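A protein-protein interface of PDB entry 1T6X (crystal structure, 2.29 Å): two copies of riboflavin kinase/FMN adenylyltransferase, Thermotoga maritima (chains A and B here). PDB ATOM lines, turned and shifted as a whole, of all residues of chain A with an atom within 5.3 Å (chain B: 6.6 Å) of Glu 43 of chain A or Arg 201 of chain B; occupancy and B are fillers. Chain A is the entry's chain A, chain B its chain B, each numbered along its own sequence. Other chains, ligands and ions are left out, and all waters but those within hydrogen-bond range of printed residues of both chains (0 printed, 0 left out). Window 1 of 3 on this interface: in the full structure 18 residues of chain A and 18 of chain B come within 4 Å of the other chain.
The side-chain amino group of Lys 209 of chain B is in salt-bridge range of the side-chain carboxylate of Asp 48 of chain A (3.1 Å).
OD2 of Asp 48 of chain A lies within salt-bridge range of NH1 of Arg 201 of chain B (3.1 Å).
The side-chain amino group (NZ) of Lys 209 of chain B lies within salt-bridge range of the side-chain carboxylate (OE2) of Glu 249 of chain B (3.6 Å).
N of Arg 201 of chain B is in hydrogen-bond range of O of Glu 249 of chain B.
Among the printed residues, merely in contact across the chains: Pro 42 of chain A with Ile 285 of chain B, Glu 43 of chain A with Arg 201 of chain B, Leu 46 of chain A with Arg 201 of chain B and Leu 46 of chain A with Phe 211 of chain B.
Glu 43 of chain A touches just one residue of chain B: Arg 201.
Printed residues of chain B within 4 Å of Leu 46 of chain A: Arg 201 (3.8 Å) and Phe 211 (3.96 Å).
Of the printed residues of chain B, Asp 48 of chain A touches Arg 201 (3.1 Å) and Lys 209 (3.1 Å).
Leu 199 of chain B touches none of the printed residues of chain A.
Arg 201 of chain B touches just these residues of chain A: Glu 43 (3.6 Å), Leu 46 (3.8 Å) and Asp 48 (3.1 Å).
Of the printed residues of chain A, Lys 209 of chain B touches Asp 48.
Lys 210 of chain B touches none of the printed residues of chain A.
Of the printed residues of chain A, Phe 211 of chain B touches Leu 46 (3.96 Å).
Of the printed residues of chain A, Ile 285 of chain B touches Pro 42 (3.6 Å).
The nearest printed residue of chain A that does not touch Arg 201 of chain B is Phe 49 of chain A (6.3 Å).
The nearest printed residue of chain B that does not touch Leu 46 of chain A is Ile 285 of chain B (4.8 Å).
Of the 8 printed residues of chain A, 4 touch a printed residue of chain B.
Along chain A the printed residues that touch a printed residue of chain B span positions 42 to 48.
Among the printed residues, Asp or Glu carboxylates within 4 Å of a Lys or Arg side-chain nitrogen of the other chain: Asp 48 of chain A with Arg 201 of chain B and Asp 48 of chain A with Lys 209 of chain B.
No position is printed for both chains.
Of the 6 pairs that touch across the chains among the printed residues, none has its exchanged pair printed and touching as well.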
ATOM      1  N   PRO A  41      24.185  12.344 -16.252  1.00  0.00           N
ATOM      2  CA  PRO A  41      25.278  13.177 -15.773  1.00  0.00           C
ATOM      3  C   PRO A  41      24.768  13.736 -14.446  1.00  0.00           C
ATOM      4  O   PRO A  41      23.566  13.741 -14.185  1.00  0.00           O
ATOM      5  CB  PRO A  41      25.416  14.223 -16.875  1.00  0.00           C
ATOM      6  CG  PRO A  41      24.035  14.372 -17.393  1.00  0.00           C
ATOM      7  CD  PRO A  41      23.538  12.945 -17.432  1.00  0.00           C
ATOM      8  N   PRO A  42      25.660  14.214 -13.588  1.00  0.00           N
ATOM      9  CA  PRO A  42      25.212  14.743 -12.294  1.00  0.00           C
ATOM     10  C   PRO A  42      24.270  15.943 -12.405  1.00  0.00           C
ATOM     11  O   PRO A  42      23.375  16.115 -11.580  1.00  0.00           O
ATOM     12  CB  PRO A  42      26.517  15.120 -11.595  1.00  0.00           C
ATOM     13  CG  PRO A  42      27.571  14.339 -12.343  1.00  0.00           C
ATOM     14  CD  PRO A  42      27.100  14.421 -13.771  1.00  0.00           C
ATOM     15  N   GLU A  43      24.497  16.776 -13.418  1.00  0.00           N
ATOM     16  CA  GLU A  43      23.690  17.972 -13.643  1.00  0.00           C
ATOM     17  C   GLU A  43      22.242  17.599 -13.868  1.00  0.00           C
ATOM     18  O   GLU A  43      21.357  18.372 -13.569  1.00  0.00           O
ATOM     19  CB  GLU A  43      24.199  18.750 -14.870  1.00  0.00           C
ATOM     20  CG  GLU A  43      25.650  19.218 -14.789  1.00  0.00           C
ATOM     21  CD  GLU A  43      26.658  18.101 -15.062  1.00  0.00           C
ATOM     22  OE1 GLU A  43      27.777  18.159 -14.512  1.00  0.00           O
ATOM     23  OE2 GLU A  43      26.337  17.178 -15.837  1.00  0.00           O
ATOM     24  N   TYR A  44      22.020  16.405 -14.405  1.00  0.00           N
ATOM     25  CA  TYR A  44      20.683  15.917 -14.703  1.00  0.00           C
ATOM     26  C   TYR A  44      19.670  16.089 -13.573  1.00  0.00           C
ATOM     27  O   TYR A  44      18.482  16.232 -13.832  1.00  0.00           O
ATOM     28  CB  TYR A  44      20.754  14.438 -15.109  1.00  0.00           C
ATOM     29  CG  TYR A  44      19.416  13.765 -15.390  1.00  0.00           C
ATOM     30  CD1 TYR A  44      18.942  13.619 -16.686  1.00  0.00           C
ATOM     31  CD2 TYR A  44      18.653  13.235 -14.349  1.00  0.00           C
ATOM     32  CE1 TYR A  44      17.742  12.950 -16.946  1.00  0.00           C
ATOM     33  CE2 TYR A  44      17.455  12.571 -14.585  1.00  0.00           C
ATOM     34  CZ  TYR A  44      17.003  12.426 -15.882  1.00  0.00           C
ATOM     35  OH  TYR A  44      15.818  11.739 -16.105  1.00  0.00           O
ATOM     36  N   PHE A  45      20.117  16.099 -12.332  1.00  0.00           N
ATOM     37  CA  PHE A  45      19.176  16.221 -11.237  1.00  0.00           C
ATOM     38  C   PHE A  45      18.908  17.643 -10.782  1.00  0.00           C
ATOM     39  O   PHE A  45      17.982  17.905  -9.996  1.00  0.00           O
ATOM     40  CB  PHE A  45      19.648  15.321 -10.095  1.00  0.00           C
ATOM     41  CG  PHE A  45      19.638  13.880 -10.483  1.00  0.00           C
ATOM     42  CD1 PHE A  45      18.442  13.161 -10.481  1.00  0.00           C
ATOM     43  CD2 PHE A  45      20.776  13.297 -11.044  1.00  0.00           C
ATOM     44  CE1 PHE A  45      18.369  11.901 -11.041  1.00  0.00           C
ATOM     45  CE2 PHE A  45      20.718  12.032 -11.609  1.00  0.00           C
ATOM     46  CZ  PHE A  45      19.508  11.331 -11.611  1.00  0.00           C
ATOM     47  N   LEU A  46      19.713  18.570 -11.288  1.00  0.00           N
ATOM     48  CA  LEU A  46      19.530  19.980 -10.970  1.00  0.00           C
ATOM     49  C   LEU A  46      18.363  20.557 -11.779  1.00  0.00           C
ATOM     50  O   LEU A  46      18.047  20.084 -12.877  1.00  0.00           O
ATOM     51  CB  LEU A  46      20.816  20.747 -11.261  1.00  0.00           C
ATOM     52  CG  LEU A  46      21.974  20.193 -10.435  1.00  0.00           C
ATOM     53  CD1 LEU A  46      23.248  20.969 -10.721  1.00  0.00           C
ATOM     54  CD2 LEU A  46      21.599  20.259  -8.951  1.00  0.00           C
ATOM     55  N   ASP A  48      17.851  23.494 -13.516  1.00  0.00           N
ATOM     56  CA  ASP A  48      18.137  24.102 -14.823  1.00  0.00           C
ATOM     57  C   ASP A  48      18.706  23.181 -15.908  1.00  0.00           C
ATOM     58  O   ASP A  48      19.154  23.661 -16.949  1.00  0.00           O
ATOM     59  CB  ASP A  48      19.104  25.263 -14.641  1.00  0.00           C
ATOM     60  CG  ASP A  48      20.370  24.839 -13.930  1.00  0.00           C
ATOM     61  OD1 ASP A  48      20.548  23.612 -13.752  1.00  0.00           O
ATOM     62  OD2 ASP A  48      21.181  25.718 -13.552  1.00  0.00           O
ATOM     63  N   PHE A  49      18.697  21.873 -15.678  1.00  0.00           N
ATOM     64  CA  PHE A  49      19.233  20.947 -16.660  1.00  0.00           C
ATOM     65  C   PHE A  49      18.395  20.968 -17.922  1.00  0.00           C
ATOM     66  O   PHE A  49      17.243  20.596 -17.903  1.00  0.00           O
ATOM     67  CB  PHE A  49      19.271  19.536 -16.069  1.00  0.00           C
ATOM     68  CG  PHE A  49      19.971  18.543 -16.929  1.00  0.00           C
ATOM     69  CD1 PHE A  49      21.315  18.704 -17.230  1.00  0.00           C
ATOM     70  CD2 PHE A  49      19.269  17.485 -17.497  1.00  0.00           C
ATOM     71  CE1 PHE A  49      21.954  17.838 -18.091  1.00  0.00           C
ATOM     72  CE2 PHE A  49      19.892  16.598 -18.361  1.00  0.00           C
ATOM     73  CZ  PHE A  49      21.239  16.777 -18.665  1.00  0.00           C
ATOM     74  N   LEU B 199      31.077  29.343  -3.514  1.00  0.00           N
ATOM     75  CA  LEU B 199      30.945  28.257  -4.485  1.00  0.00           C
ATOM     76  C   LEU B 199      29.990  28.831  -5.539  1.00  0.00           C
ATOM     77  O   LEU B 199      28.917  29.329  -5.190  1.00  0.00           O
ATOM     78  CB  LEU B 199      30.287  27.029  -3.868  1.00  0.00           C
ATOM     79  CG  LEU B 199      29.889  25.939  -4.874  1.00  0.00           C
ATOM     80  CD1 LEU B 199      31.121  25.185  -5.309  1.00  0.00           C
ATOM     81  CD2 LEU B 199      28.883  24.983  -4.244  1.00  0.00           C
ATOM     82  N   VAL B 200      30.363  28.769  -6.813  1.00  0.00           N
ATOM     83  CA  VAL B 200      29.507  29.307  -7.870  1.00  0.00           C
ATOM     84  C   VAL B 200      29.153  28.324  -8.957  1.00  0.00           C
ATOM     85  O   VAL B 200      29.768  27.279  -9.066  1.00  0.00           O
ATOM     86  CB  VAL B 200      30.158  30.506  -8.598  1.00  0.00           C
ATOM     87  CG1 VAL B 200      30.451  31.634  -7.597  1.00  0.00           C
ATOM     88  CG2 VAL B 200      31.423  30.050  -9.340  1.00  0.00           C
ATOM     89  N   ARG B 201      28.135  28.658  -9.745  1.00  0.00           N
ATOM     90  CA  ARG B 201      27.768  27.836 -10.890  1.00  0.00           C
ATOM     91  C   ARG B 201      28.206  28.724 -12.052  1.00  0.00           C
ATOM     92  O   ARG B 201      27.653  29.799 -12.251  1.00  0.00           O
ATOM     93  CB  ARG B 201      26.271  27.598 -10.989  1.00  0.00           C
ATOM     94  CG  ARG B 201      25.917  26.516 -12.009  1.00  0.00           C
ATOM     95  CD  ARG B 201      26.183  25.147 -11.415  1.00  0.00           C
ATOM     96  NE  ARG B 201      26.017  24.038 -12.356  1.00  0.00           N
ATOM     97  CZ  ARG B 201      24.864  23.631 -12.880  1.00  0.00           C
ATOM     98  NH1 ARG B 201      23.720  24.233 -12.574  1.00  0.00           N
ATOM     99  NH2 ARG B 201      24.862  22.605 -13.710  1.00  0.00           N
ATOM    100  N   VAL B 202      29.213  28.274 -12.788  1.00  0.00           N
ATOM    101  CA  VAL B 202      29.765  29.023 -13.898  1.00  0.00           C
ATOM    102  C   VAL B 202      29.078  28.651 -15.203  1.00  0.00           C
ATOM    103  O   VAL B 202      29.069  27.490 -15.608  1.00  0.00           O
ATOM    104  CB  VAL B 202      31.277  28.731 -14.036  1.00  0.00           C
ATOM    105  CG1 VAL B 202      31.879  29.573 -15.124  1.00  0.00           C
ATOM    106  CG2 VAL B 202      31.991  28.984 -12.714  1.00  0.00           C
ATOM    107  N   HIS B 203      28.483  29.642 -15.853  1.00  0.00           N
ATOM    108  CA  HIS B 203      27.837  29.435 -17.132  1.00  0.00           C
ATOM    109  C   HIS B 203      28.893  29.862 -18.171  1.00  0.00           C
ATOM    110  O   HIS B 203      29.198  31.040 -18.297  1.00  0.00           O
ATOM    111  CB  HIS B 203      26.592  30.312 -17.241  1.00  0.00           C
ATOM    112  CG  HIS B 203      25.752  30.011 -18.438  1.00  0.00           C
ATOM    113  ND1 HIS B 203      26.279  29.905 -19.708  1.00  0.00           N
ATOM    114  CD2 HIS B 203      24.424  29.790 -18.563  1.00  0.00           C
ATOM    115  CE1 HIS B 203      25.311  29.631 -20.562  1.00  0.00           C
ATOM    116  NE2 HIS B 203      24.175  29.556 -19.893  1.00  0.00           N
ATOM    117  N   LYS B 209      27.860  24.319 -18.205  1.00  0.00           N
ATOM    118  CA  LYS B 209      27.829  24.732 -16.815  1.00  0.00           C
ATOM    119  C   LYS B 209      28.739  23.888 -15.940  1.00  0.00           C
ATOM    120  O   LYS B 209      28.638  22.664 -15.912  1.00  0.00           O
ATOM    121  CB  LYS B 209      26.408  24.699 -16.268  1.00  0.00           C
ATOM    122  CG  LYS B 209      25.616  25.907 -16.721  1.00  0.00           C
ATOM    123  CD  LYS B 209      24.343  26.123 -15.950  1.00  0.00           C
ATOM    124  CE  LYS B 209      23.688  27.421 -16.387  1.00  0.00           C
ATOM    125  NZ  LYS B 209      22.411  27.672 -15.652  1.00  0.00           N
ATOM    126  N   LYS B 210      29.652  24.552 -15.239  1.00  0.00           N
ATOM    127  CA  LYS B 210      30.572  23.883 -14.331  1.00  0.00           C
ATOM    128  C   LYS B 210      30.357  24.575 -13.008  1.00  0.00           C
ATOM    129  O   LYS B 210      29.510  25.444 -12.910  1.00  0.00           O
ATOM    130  CB  LYS B 210      32.028  24.085 -14.765  1.00  0.00           C
ATOM    131  CG  LYS B 210      32.420  23.408 -16.080  1.00  0.00           C
ATOM    132  CD  LYS B 210      31.900  21.981 -16.121  1.00  0.00           C
ATOM    133  CE  LYS B 210      32.418  21.206 -17.313  1.00  0.00           C
ATOM    134  NZ  LYS B 210      33.687  20.506 -17.001  1.00  0.00           N
ATOM    135  N   PHE B 211      31.101  24.175 -11.985  1.00  0.00           N
ATOM    136  CA  PHE B 211      31.011  24.807 -10.688  1.00  0.00           C
ATOM    137  C   PHE B 211      32.355  25.487 -10.525  1.00  0.00           C
ATOM    138  O   PHE B 211      33.313  25.138 -11.211  1.00  0.00           O
ATOM    139  CB  PHE B 211      30.798  23.772  -9.592  1.00  0.00           C
ATOM    140  CG  PHE B 211      29.386  23.235  -9.518  1.00  0.00           C
ATOM    141  CD1 PHE B 211      28.445  23.820  -8.668  1.00  0.00           C
ATOM    142  CD2 PHE B 211      28.999  22.135 -10.290  1.00  0.00           C
ATOM    143  CE1 PHE B 211      27.131  23.307  -8.588  1.00  0.00           C
ATOM    144  CE2 PHE B 211      27.701  21.619 -10.225  1.00  0.00           C
ATOM    145  CZ  PHE B 211      26.764  22.201  -9.374  1.00  0.00           C
ATOM    146  N   GLY B 212      32.439  26.472  -9.639  1.00  0.00           N
ATOM    147  CA  GLY B 212      33.698  27.151  -9.450  1.00  0.00           C
ATOM    148  C   GLY B 212      33.796  27.565  -8.017  1.00  0.00           C
ATOM    149  O   GLY B 212      32.845  27.404  -7.251  1.00  0.00           O
ATOM    150  N   LYS B 247      28.888  34.103 -16.709  1.00  0.00           N
ATOM    151  CA  LYS B 247      27.791  34.478 -15.823  1.00  0.00           C
ATOM    152  C   LYS B 247      28.007  33.532 -14.662  1.00  0.00           C
ATOM    153  O   LYS B 247      28.234  32.364 -14.883  1.00  0.00           O
ATOM    154  CB  LYS B 247      26.428  34.204 -16.462  1.00  0.00           C
ATOM    155  CG  LYS B 247      26.048  35.141 -17.596  1.00  0.00           C
ATOM    156  CD  LYS B 247      24.576  34.978 -17.965  1.00  0.00           C
ATOM    157  CE  LYS B 247      24.159  35.890 -19.121  1.00  0.00           C
ATOM    158  NZ  LYS B 247      24.790  35.531 -20.423  1.00  0.00           N
ATOM    159  N   LEU B 248      27.941  34.020 -13.434  1.00  0.00           N
ATOM    160  CA  LEU B 248      28.181  33.171 -12.279  1.00  0.00           C
ATOM    161  C   LEU B 248      27.101  33.270 -11.239  1.00  0.00           C
ATOM    162  O   LEU B 248      26.907  34.339 -10.681  1.00  0.00           O
ATOM    163  CB  LEU B 248      29.477  33.579 -11.580  1.00  0.00           C
ATOM    164  CG  LEU B 248      30.778  33.748 -12.353  1.00  0.00           C
ATOM    165  CD1 LEU B 248      31.853  34.272 -11.410  1.00  0.00           C
ATOM    166  CD2 LEU B 248      31.211  32.410 -12.954  1.00  0.00           C
ATOM    167  N   GLU B 249      26.411  32.171 -10.953  1.00  0.00           N
ATOM    168  CA  GLU B 249      25.405  32.175  -9.897  1.00  0.00           C
ATOM    169  C   GLU B 249      26.161  31.915  -8.584  1.00  0.00           C
ATOM    170  O   GLU B 249      26.898  30.938  -8.451  1.00  0.00           O
ATOM    171  CB  GLU B 249      24.386  31.070 -10.120  1.00  0.00           C
ATOM    172  CG  GLU B 249      23.757  31.085 -11.482  1.00  0.00           C
ATOM    173  CD  GLU B 249      22.978  29.815 -11.762  1.00  0.00           C
ATOM    174  OE1 GLU B 249      21.864  29.652 -11.216  1.00  0.00           O
ATOM    175  OE2 GLU B 249      23.498  28.967 -12.521  1.00  0.00           O
ATOM    176  N   VAL B 250      25.988  32.790  -7.613  1.00  0.00           N
ATOM    177  CA  VAL B 250      26.672  32.637  -6.344  1.00  0.00           C
ATOM    178  C   VAL B 250      25.772  31.776  -5.490  1.00  0.00           C
ATOM    179  O   VAL B 250      24.701  32.207  -5.072  1.00  0.00           O
ATOM    180  CB  VAL B 250      26.895  33.995  -5.678  1.00  0.00           C
ATOM    181  CG1 VAL B 250      27.839  33.843  -4.512  1.00  0.00           C
ATOM    182  CG2 VAL B 250      27.472  34.972  -6.680  1.00  0.00           C
ATOM    183  N   LEU B 251      26.222  30.552  -5.229  1.00  0.00           N
ATOM    184  CA  LEU B 251      25.430  29.589  -4.491  1.00  0.00           C
ATOM    185  C   LEU B 251      25.586  29.603  -2.996  1.00  0.00           C
ATOM    186  O   LEU B 251      24.604  29.511  -2.273  1.00  0.00           O
ATOM    187  CB  LEU B 251      25.715  28.185  -5.017  1.00  0.00           C
ATOM    188  CG  LEU B 251      25.642  27.967  -6.540  1.00  0.00           C
ATOM    189  CD1 LEU B 251      25.711  26.473  -6.814  1.00  0.00           C
ATOM    190  CD2 LEU B 251      24.354  28.536  -7.123  1.00  0.00           C
ATOM    191  N   ILE B 285      23.601  17.838  -5.180  1.00  0.00           N
ATOM    192  CA  ILE B 285      23.140  16.766  -6.055  1.00  0.00           C
ATOM    193  C   ILE B 285      22.305  15.710  -5.327  1.00  0.00           C
ATOM    194  O   ILE B 285      21.351  15.187  -5.885  1.00  0.00           O
ATOM    195  CB  ILE B 285      24.340  16.037  -6.719  1.00  0.00           C
ATOM    196  CG1 ILE B 285      25.002  16.937  -7.762  1.00  0.00           C
ATOM    197  CG2 ILE B 285      23.871  14.745  -7.362  1.00  0.00           C
ATOM    198  CD1 ILE B 285      26.315  16.367  -8.267  1.00  0.00           C
